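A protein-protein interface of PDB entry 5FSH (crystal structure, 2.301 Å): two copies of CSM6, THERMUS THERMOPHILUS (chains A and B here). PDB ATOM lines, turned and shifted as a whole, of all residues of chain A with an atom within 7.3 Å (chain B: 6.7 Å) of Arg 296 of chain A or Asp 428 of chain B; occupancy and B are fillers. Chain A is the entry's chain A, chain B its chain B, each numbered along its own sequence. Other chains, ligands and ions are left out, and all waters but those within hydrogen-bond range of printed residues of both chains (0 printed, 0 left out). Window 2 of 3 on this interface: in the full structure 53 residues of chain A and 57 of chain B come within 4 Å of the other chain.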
ATOM      1  N   LEU A 246     -17.563  25.026  -1.055  1.00  0.00           N
ATOM      2  CA  LEU A 246     -18.768  25.365  -1.811  1.00  0.00           C
ATOM      3  C   LEU A 246     -19.055  24.371  -2.935  1.00  0.00           C
ATOM      4  O   LEU A 246     -19.700  24.720  -3.922  1.00  0.00           O
ATOM      5  CB  LEU A 246     -18.696  26.788  -2.380  1.00  0.00           C
ATOM      6  CG  LEU A 246     -18.514  27.919  -1.375  1.00  0.00           C
ATOM      7  CD1 LEU A 246     -18.183  29.215  -2.103  1.00  0.00           C
ATOM      8  CD2 LEU A 246     -19.778  28.052  -0.517  1.00  0.00           C
ATOM      9  N   ASP A 290     -28.114  21.985  -2.852  1.00  0.00           N
ATOM     10  CA  ASP A 290     -27.862  21.421  -4.178  1.00  0.00           C
ATOM     11  C   ASP A 290     -29.062  21.634  -5.097  1.00  0.00           C
ATOM     12  O   ASP A 290     -28.929  22.095  -6.244  1.00  0.00           O
ATOM     13  CB  ASP A 290     -27.531  19.931  -4.044  1.00  0.00           C
ATOM     14  CG  ASP A 290     -27.381  19.242  -5.385  1.00  0.00           C
ATOM     15  OD1 ASP A 290     -26.398  19.532  -6.092  1.00  0.00           O
ATOM     16  OD2 ASP A 290     -28.243  18.405  -5.730  1.00  0.00           O
ATOM     17  N   ARG A 291     -30.254  21.343  -4.581  1.00  0.00           N
ATOM     18  CA  ARG A 291     -31.472  21.494  -5.369  1.00  0.00           C
ATOM     19  C   ARG A 291     -31.748  22.953  -5.710  1.00  0.00           C
ATOM     20  O   ARG A 291     -32.143  23.263  -6.839  1.00  0.00           O
ATOM     21  CB  ARG A 291     -32.642  20.887  -4.609  1.00  0.00           C
ATOM     22  CG  ARG A 291     -34.000  21.207  -5.171  1.00  0.00           C
ATOM     23  CD  ARG A 291     -35.036  20.639  -4.229  1.00  0.00           C
ATOM     24  NE  ARG A 291     -36.399  20.751  -4.742  1.00  0.00           N
ATOM     25  CZ  ARG A 291     -37.453  20.204  -4.142  1.00  0.00           C
ATOM     26  NH1 ARG A 291     -37.297  19.518  -3.018  1.00  0.00           N
ATOM     27  NH2 ARG A 291     -38.666  20.343  -4.675  1.00  0.00           N
ATOM     28  N   PHE A 292     -31.560  23.862  -4.749  1.00  0.00           N
ATOM     29  CA  PHE A 292     -31.750  25.276  -5.054  1.00  0.00           C
ATOM     30  C   PHE A 292     -30.724  25.779  -6.066  1.00  0.00           C
ATOM     31  O   PHE A 292     -31.033  26.660  -6.879  1.00  0.00           O
ATOM     32  CB  PHE A 292     -31.702  26.108  -3.774  1.00  0.00           C
ATOM     33  CG  PHE A 292     -31.397  27.554  -4.013  1.00  0.00           C
ATOM     34  CD1 PHE A 292     -32.360  28.399  -4.535  1.00  0.00           C
ATOM     35  CD2 PHE A 292     -30.144  28.068  -3.729  1.00  0.00           C
ATOM     36  CE1 PHE A 292     -32.078  29.732  -4.765  1.00  0.00           C
ATOM     37  CE2 PHE A 292     -29.857  29.398  -3.956  1.00  0.00           C
ATOM     38  CZ  PHE A 292     -30.824  30.231  -4.471  1.00  0.00           C
ATOM     39  N   LEU A 293     -29.506  25.235  -6.043  1.00  0.00           N
ATOM     40  CA  LEU A 293     -28.524  25.608  -7.054  1.00  0.00           C
ATOM     41  C   LEU A 293     -28.983  25.170  -8.437  1.00  0.00           C
ATOM     42  O   LEU A 293     -28.817  25.912  -9.410  1.00  0.00           O
ATOM     43  CB  LEU A 293     -27.149  25.015  -6.728  1.00  0.00           C
ATOM     44  CG  LEU A 293     -26.356  25.653  -5.579  1.00  0.00           C
ATOM     45  CD1 LEU A 293     -25.072  24.880  -5.336  1.00  0.00           C
ATOM     46  CD2 LEU A 293     -26.060  27.118  -5.857  1.00  0.00           C
ATOM     47  N   LYS A 294     -29.575  23.975  -8.542  1.00  0.00           N
ATOM     48  CA  LYS A 294     -30.126  23.545  -9.828  1.00  0.00           C
ATOM     49  C   LYS A 294     -31.342  24.379 -10.230  1.00  0.00           C
ATOM     50  O   LYS A 294     -31.532  24.679 -11.415  1.00  0.00           O
ATOM     51  CB  LYS A 294     -30.503  22.063  -9.772  1.00  0.00           C
ATOM     52  CG  LYS A 294     -29.382  21.113 -10.160  1.00  0.00           C
ATOM     53  CD  LYS A 294     -29.362  19.897  -9.244  1.00  0.00           C
ATOM     54  CE  LYS A 294     -28.214  18.970  -9.609  1.00  0.00           C
ATOM     55  NZ  LYS A 294     -28.250  17.697  -8.831  1.00  0.00           N
ATOM     56  N   ALA A 295     -32.179  24.761  -9.259  1.00  0.00           N
ATOM     57  CA  ALA A 295     -33.481  25.358  -9.541  1.00  0.00           C
ATOM     58  C   ALA A 295     -33.434  26.876  -9.677  1.00  0.00           C
ATOM     59  O   ALA A 295     -34.193  27.446 -10.471  1.00  0.00           O
ATOM     60  CB  ALA A 295     -34.476  24.983  -8.435  1.00  0.00           C
ATOM     61  N   ARG A 296     -32.566  27.543  -8.911  1.00  0.00           N
ATOM     62  CA  ARG A 296     -32.521  29.000  -8.797  1.00  0.00           C
ATOM     63  C   ARG A 296     -33.858  29.587  -8.354  1.00  0.00           C
ATOM     64  O   ARG A 296     -34.187  30.724  -8.702  1.00  0.00           O
ATOM     65  CB  ARG A 296     -32.062  29.658 -10.107  1.00  0.00           C
ATOM     66  CG  ARG A 296     -31.097  28.809 -10.918  1.00  0.00           C
ATOM     67  CD  ARG A 296     -30.241  29.653 -11.833  1.00  0.00           C
ATOM     68  NE  ARG A 296     -29.494  28.830 -12.779  1.00  0.00           N
ATOM     69  CZ  ARG A 296     -28.458  28.066 -12.446  1.00  0.00           C
ATOM     70  NH1 ARG A 296     -28.048  28.012 -11.188  1.00  0.00           N
ATOM     71  NH2 ARG A 296     -27.834  27.349 -13.369  1.00  0.00           N
ATOM     72  N   ASP A 297     -34.640  28.827  -7.593  1.00  0.00           N
ATOM     73  CA  ASP A 297     -35.955  29.252  -7.129  1.00  0.00           C
ATOM     74  C   ASP A 297     -35.833  29.739  -5.691  1.00  0.00           C
ATOM     75  O   ASP A 297     -35.487  28.964  -4.794  1.00  0.00           O
ATOM     76  CB  ASP A 297     -36.963  28.107  -7.226  1.00  0.00           C
ATOM     77  CG  ASP A 297     -38.390  28.546  -6.931  1.00  0.00           C
ATOM     78  OD1 ASP A 297     -38.598  29.651  -6.385  1.00  0.00           O
ATOM     79  OD2 ASP A 297     -39.314  27.769  -7.242  1.00  0.00           O
ATOM     80  N   PHE A 298     -36.129  31.013  -5.468  1.00  0.00           N
ATOM     81  CA  PHE A 298     -35.999  31.553  -4.124  1.00  0.00           C
ATOM     82  C   PHE A 298     -37.181  31.205  -3.228  1.00  0.00           C
ATOM     83  O   PHE A 298     -37.258  31.720  -2.110  1.00  0.00           O
ATOM     84  CB  PHE A 298     -35.794  33.068  -4.189  1.00  0.00           C
ATOM     85  CG  PHE A 298     -34.407  33.470  -4.607  1.00  0.00           C
ATOM     86  CD1 PHE A 298     -33.984  33.305  -5.918  1.00  0.00           C
ATOM     87  CD2 PHE A 298     -33.522  34.007  -3.688  1.00  0.00           C
ATOM     88  CE1 PHE A 298     -32.703  33.672  -6.301  1.00  0.00           C
ATOM     89  CE2 PHE A 298     -32.242  34.375  -4.067  1.00  0.00           C
ATOM     90  CZ  PHE A 298     -31.833  34.207  -5.375  1.00  0.00           C
ATOM     91  N   ALA A 299     -38.094  30.342  -3.682  1.00  0.00           N
ATOM     92  CA  ALA A 299     -39.151  29.858  -2.800  1.00  0.00           C
ATOM     93  C   ALA A 299     -38.601  28.855  -1.791  1.00  0.00           C
ATOM     94  O   ALA A 299     -38.975  28.879  -0.611  1.00  0.00           O
ATOM     95  CB  ALA A 299     -40.284  29.237  -3.618  1.00  0.00           C
ATOM     96  N   LEU A 300     -37.708  27.965  -2.233  1.00  0.00           N
ATOM     97  CA  LEU A 300     -37.069  27.017  -1.328  1.00  0.00           C
ATOM     98  C   LEU A 300     -36.209  27.781  -0.326  1.00  0.00           C
ATOM     99  O   LEU A 300     -35.035  28.054  -0.588  1.00  0.00           O
ATOM    100  CB  LEU A 300     -36.220  25.995  -2.095  1.00  0.00           C
ATOM    101  CG  LEU A 300     -36.578  25.580  -3.526  1.00  0.00           C
ATOM    102  CD1 LEU A 300     -35.433  25.928  -4.465  1.00  0.00           C
ATOM    103  CD2 LEU A 300     -36.904  24.089  -3.633  1.00  0.00           C
ATOM    104  N   VAL A 304     -31.590  28.513   0.069  1.00  0.00           N
ATOM    105  CA  VAL A 304     -31.071  29.870   0.250  1.00  0.00           C
ATOM    106  C   VAL A 304     -30.393  30.011   1.608  1.00  0.00           C
ATOM    107  O   VAL A 304     -29.322  30.626   1.729  1.00  0.00           O
ATOM    108  CB  VAL A 304     -32.198  30.906   0.087  1.00  0.00           C
ATOM    109  CG1 VAL A 304     -31.651  32.327   0.216  1.00  0.00           C
ATOM    110  CG2 VAL A 304     -32.921  30.706  -1.241  1.00  0.00           C
ATOM    111  N   VAL B 324     -14.310  26.526  -6.875  1.00  0.00           N
ATOM    112  CA  VAL B 324     -15.130  27.731  -7.044  1.00  0.00           C
ATOM    113  C   VAL B 324     -14.268  28.982  -6.903  1.00  0.00           C
ATOM    114  O   VAL B 324     -14.300  29.904  -7.741  1.00  0.00           O
ATOM    115  CB  VAL B 324     -16.283  27.740  -6.022  1.00  0.00           C
ATOM    116  CG1 VAL B 324     -17.059  29.039  -6.101  1.00  0.00           C
ATOM    117  CG2 VAL B 324     -17.203  26.568  -6.234  1.00  0.00           C
ATOM    118  N   TYR B 331     -10.872  33.927 -13.549  1.00  0.00           N
ATOM    119  CA  TYR B 331     -11.698  34.889 -14.275  1.00  0.00           C
ATOM    120  C   TYR B 331     -11.158  36.308 -14.131  1.00  0.00           C
ATOM    121  O   TYR B 331     -11.069  37.047 -15.120  1.00  0.00           O
ATOM    122  CB  TYR B 331     -13.148  34.828 -13.794  1.00  0.00           C
ATOM    123  CG  TYR B 331     -14.002  33.769 -14.463  1.00  0.00           C
ATOM    124  CD1 TYR B 331     -13.985  33.599 -15.845  1.00  0.00           C
ATOM    125  CD2 TYR B 331     -14.826  32.941 -13.709  1.00  0.00           C
ATOM    126  CE1 TYR B 331     -14.764  32.641 -16.448  1.00  0.00           C
ATOM    127  CE2 TYR B 331     -15.602  31.975 -14.304  1.00  0.00           C
ATOM    128  CZ  TYR B 331     -15.566  31.827 -15.669  1.00  0.00           C
ATOM    129  OH  TYR B 331     -16.339  30.864 -16.256  1.00  0.00           O
ATOM    130  N   GLY B 417     -19.537  32.286 -18.770  1.00  0.00           N
ATOM    131  CA  GLY B 417     -19.946  32.202 -17.381  1.00  0.00           C
ATOM    132  C   GLY B 417     -19.198  33.125 -16.445  1.00  0.00           C
ATOM    133  O   GLY B 417     -19.081  32.832 -15.252  1.00  0.00           O
ATOM    134  N   ARG B 418     -18.709  34.252 -16.968  1.00  0.00           N
ATOM    135  CA  ARG B 418     -17.857  35.133 -16.175  1.00  0.00           C
ATOM    136  C   ARG B 418     -18.597  35.673 -14.955  1.00  0.00           C
ATOM    137  O   ARG B 418     -18.111  35.557 -13.824  1.00  0.00           O
ATOM    138  CB  ARG B 418     -17.325  36.272 -17.043  1.00  0.00           C
ATOM    139  CG  ARG B 418     -16.188  37.052 -16.395  1.00  0.00           C
ATOM    140  CD  ARG B 418     -16.690  38.261 -15.639  1.00  0.00           C
ATOM    141  NE  ARG B 418     -15.629  38.904 -14.877  1.00  0.00           N
ATOM    142  CZ  ARG B 418     -15.204  38.474 -13.694  1.00  0.00           C
ATOM    143  NH1 ARG B 418     -15.751  37.398 -13.141  1.00  0.00           N
ATOM    144  NH2 ARG B 418     -14.231  39.120 -13.061  1.00  0.00           N
ATOM    145  N   ASN B 419     -19.759  36.295 -15.162  1.00  0.00           N
ATOM    146  CA  ASN B 419     -20.603  36.707 -14.047  1.00  0.00           C
ATOM    147  C   ASN B 419     -21.589  35.620 -13.629  1.00  0.00           C
ATOM    148  O   ASN B 419     -22.307  35.797 -12.645  1.00  0.00           O
ATOM    149  CB  ASN B 419     -21.354  38.014 -14.374  1.00  0.00           C
ATOM    150  CG  ASN B 419     -20.458  39.260 -14.275  1.00  0.00           C
ATOM    151  OD1 ASN B 419     -20.468  40.006 -13.270  1.00  0.00           O
ATOM    152  ND2 ASN B 419     -19.687  39.495 -15.327  1.00  0.00           N
ATOM    153  N   SER B 420     -21.610  34.482 -14.317  1.00  0.00           N
ATOM    154  CA  SER B 420     -22.534  33.410 -13.969  1.00  0.00           C
ATOM    155  C   SER B 420     -22.031  32.522 -12.829  1.00  0.00           C
ATOM    156  O   SER B 420     -22.801  31.699 -12.320  1.00  0.00           O
ATOM    157  CB  SER B 420     -22.819  32.561 -15.213  1.00  0.00           C
ATOM    158  OG  SER B 420     -23.588  31.419 -14.904  1.00  0.00           O
ATOM    159  N   ALA B 421     -20.777  32.671 -12.402  1.00  0.00           N
ATOM    160  CA  ALA B 421     -20.226  31.788 -11.383  1.00  0.00           C
ATOM    161  C   ALA B 421     -20.854  32.052 -10.017  1.00  0.00           C
ATOM    162  O   ALA B 421     -21.352  33.142  -9.730  1.00  0.00           O
ATOM    163  CB  ALA B 421     -18.712  31.949 -11.301  1.00  0.00           C
ATOM    164  N   LEU B 422     -20.812  31.027  -9.164  1.00  0.00           N
ATOM    165  CA  LEU B 422     -21.452  31.107  -7.853  1.00  0.00           C
ATOM    166  C   LEU B 422     -20.949  32.300  -7.053  1.00  0.00           C
ATOM    167  O   LEU B 422     -21.726  32.954  -6.355  1.00  0.00           O
ATOM    168  CB  LEU B 422     -21.214  29.815  -7.072  1.00  0.00           C
ATOM    169  CG  LEU B 422     -21.610  29.853  -5.600  1.00  0.00           C
ATOM    170  CD1 LEU B 422     -23.112  30.056  -5.426  1.00  0.00           C
ATOM    171  CD2 LEU B 422     -21.161  28.575  -4.929  1.00  0.00           C
ATOM    172  N   LEU B 423     -19.661  32.609  -7.151  1.00  0.00           N
ATOM    173  CA  LEU B 423     -19.038  33.612  -6.297  1.00  0.00           C
ATOM    174  C   LEU B 423     -19.105  35.028  -6.867  1.00  0.00           C
ATOM    175  O   LEU B 423     -18.520  35.941  -6.283  1.00  0.00           O
ATOM    176  CB  LEU B 423     -17.584  33.222  -6.031  1.00  0.00           C
ATOM    177  CG  LEU B 423     -17.161  32.990  -4.583  1.00  0.00           C
ATOM    178  CD1 LEU B 423     -18.290  32.360  -3.809  1.00  0.00           C
ATOM    179  CD2 LEU B 423     -15.905  32.121  -4.529  1.00  0.00           C
ATOM    180  N   GLY B 426     -23.999  34.359 -10.017  1.00  0.00           N
ATOM    181  CA  GLY B 426     -24.797  33.216 -10.420  1.00  0.00           C
ATOM    182  C   GLY B 426     -24.679  32.072  -9.430  1.00  0.00           C
ATOM    183  O   GLY B 426     -24.522  32.266  -8.228  1.00  0.00           O
ATOM    184  N   PHE B 427     -24.764  30.855  -9.969  1.00  0.00           N
ATOM    185  CA  PHE B 427     -24.778  29.665  -9.131  1.00  0.00           C
ATOM    186  C   PHE B 427     -23.990  28.494  -9.701  1.00  0.00           C
ATOM    187  O   PHE B 427     -24.078  27.405  -9.135  1.00  0.00           O
ATOM    188  CB  PHE B 427     -26.226  29.216  -8.869  1.00  0.00           C
ATOM    189  CG  PHE B 427     -27.164  30.330  -8.512  1.00  0.00           C
ATOM    190  CD1 PHE B 427     -27.837  31.027  -9.501  1.00  0.00           C
ATOM    191  CD2 PHE B 427     -27.380  30.679  -7.189  1.00  0.00           C
ATOM    192  CE1 PHE B 427     -28.702  32.050  -9.181  1.00  0.00           C
ATOM    193  CE2 PHE B 427     -28.248  31.702  -6.863  1.00  0.00           C
ATOM    194  CZ  PHE B 427     -28.909  32.389  -7.861  1.00  0.00           C
ATOM    195  N   ASP B 428     -23.226  28.664 -10.777  1.00  0.00           N
ATOM    196  CA  ASP B 428     -22.545  27.533 -11.395  1.00  0.00           C
ATOM    197  C   ASP B 428     -21.392  27.033 -10.529  1.00  0.00           C
ATOM    198  O   ASP B 428     -20.671  27.819  -9.908  1.00  0.00           O
ATOM    199  CB  ASP B 428     -22.013  27.933 -12.770  1.00  0.00           C
ATOM    200  CG  ASP B 428     -23.040  28.686 -13.610  1.00  0.00           C
ATOM    201  OD1 ASP B 428     -24.260  28.531 -13.386  1.00  0.00           O
ATOM    202  OD2 ASP B 428     -22.608  29.432 -14.516  1.00  0.00           O
ATOM    203  N   VAL B 429     -21.225  25.713 -10.485  1.00  0.00           N
ATOM    204  CA  VAL B 429     -19.966  25.123 -10.033  1.00  0.00           C
ATOM    205  C   VAL B 429     -19.130  24.893 -11.285  1.00  0.00           C
ATOM    206  O   VAL B 429     -19.667  24.476 -12.323  1.00  0.00           O
ATOM    207  CB  VAL B 429     -20.179  23.826  -9.227  1.00  0.00           C
ATOM    208  CG1 VAL B 429     -18.958  22.920  -9.321  1.00  0.00           C
ATOM    209  CG2 VAL B 429     -20.456  24.151  -7.763  1.00  0.00           C
ATOM    210  N   PRO B 430     -17.833  25.183 -11.253  1.00  0.00           N
ATOM    211  CA  PRO B 430     -17.021  25.061 -12.466  1.00  0.00           C
ATOM    212  C   PRO B 430     -16.677  23.614 -12.772  1.00  0.00           C
ATOM    213  O   PRO B 430     -16.459  22.798 -11.873  1.00  0.00           O
ATOM    214  CB  PRO B 430     -15.756  25.861 -12.126  1.00  0.00           C
ATOM    215  CG  PRO B 430     -16.055  26.567 -10.834  1.00  0.00           C
ATOM    216  CD  PRO B 430     -17.068  25.751 -10.135  1.00  0.00           C
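The side-chain carboxylate of Asp 428 of chain B is in salt-bridge range of the guanidinium group of Arg 296 of chain A (3.8 Å).
The backbone NH (N) of Phe 427 of chain B sits at hydrogen-bond distance from the backbone carbonyl oxygen (O) of Ser 420 of chain B (3.2 Å).
The backbone carbonyl oxygen (O) of Asp 428 of chain B is in hydrogen-bond range of the backbone NH (N) of Leu 422 of chain B.
The backbone carbonyl oxygen (O) of Leu 293 of chain A lies within hydrogen-bond range of the guanidinium group (NH1) of Arg 296 of chain A (2.9 Å).
The side-chain hydroxyl (OG) of Ser 420 of chain B lies close to the side-chain carboxylate (OD1) of Asp 428 of chain B (3.3 Å).
Among the printed residues, pairs that only touch across the chains: Arg 296 of chain A with Phe 427 of chain B, Leu 246 of chain A with Leu 423 of chain B, Leu 293 of chain A with Phe 427 of chain B, Phe 292 of chain A with Phe 427 of chain B, Leu 246 of chain A with Val 324 of chain B, Leu 246 of chain A with Val 429 of chain B and Leu 246 of chain A with Leu 422 of chain B.
Of the printed residues of chain B, Arg 296 of chain A touches Phe 427 (3.2 Å) and Asp 428 (3.8 Å).
Printed residues of chain A within 4 Å of Asp 428 of chain B: Arg 296.
Of the printed residues of chain B, Leu 293 of chain A touches Phe 427.
Of the printed residues of chain A, Leu 423 of chain B touches Leu 246.
The nearest residue of chain B that does not touch Arg 296 of chain A is Gly 426 of chain B (5.6 Å).
The nearest printed residue of chain A that does not touch Val 324 of chain B is Leu 293 of chain A (8.1 Å).
Hydrophobic or aromatic side chains of chain A within 4 Å of the printed part of chain B: Leu 246, Phe 292 and Leu 293.
Hydrophobic or aromatic side chains of chain B that line the printed part of chain A: Val 324, Leu 422, Leu 423, Phe 427 and Val 429.
Along chain B the printed residues that touch a printed residue of chain A span positions 324 to 429.
Among the printed residues, Asp or Glu carboxylates within 4 Å of a Lys or Arg side-chain nitrogen of the other chain: Arg 296 of chain A with Asp 428 of chain B.
No position is printed for both chains.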
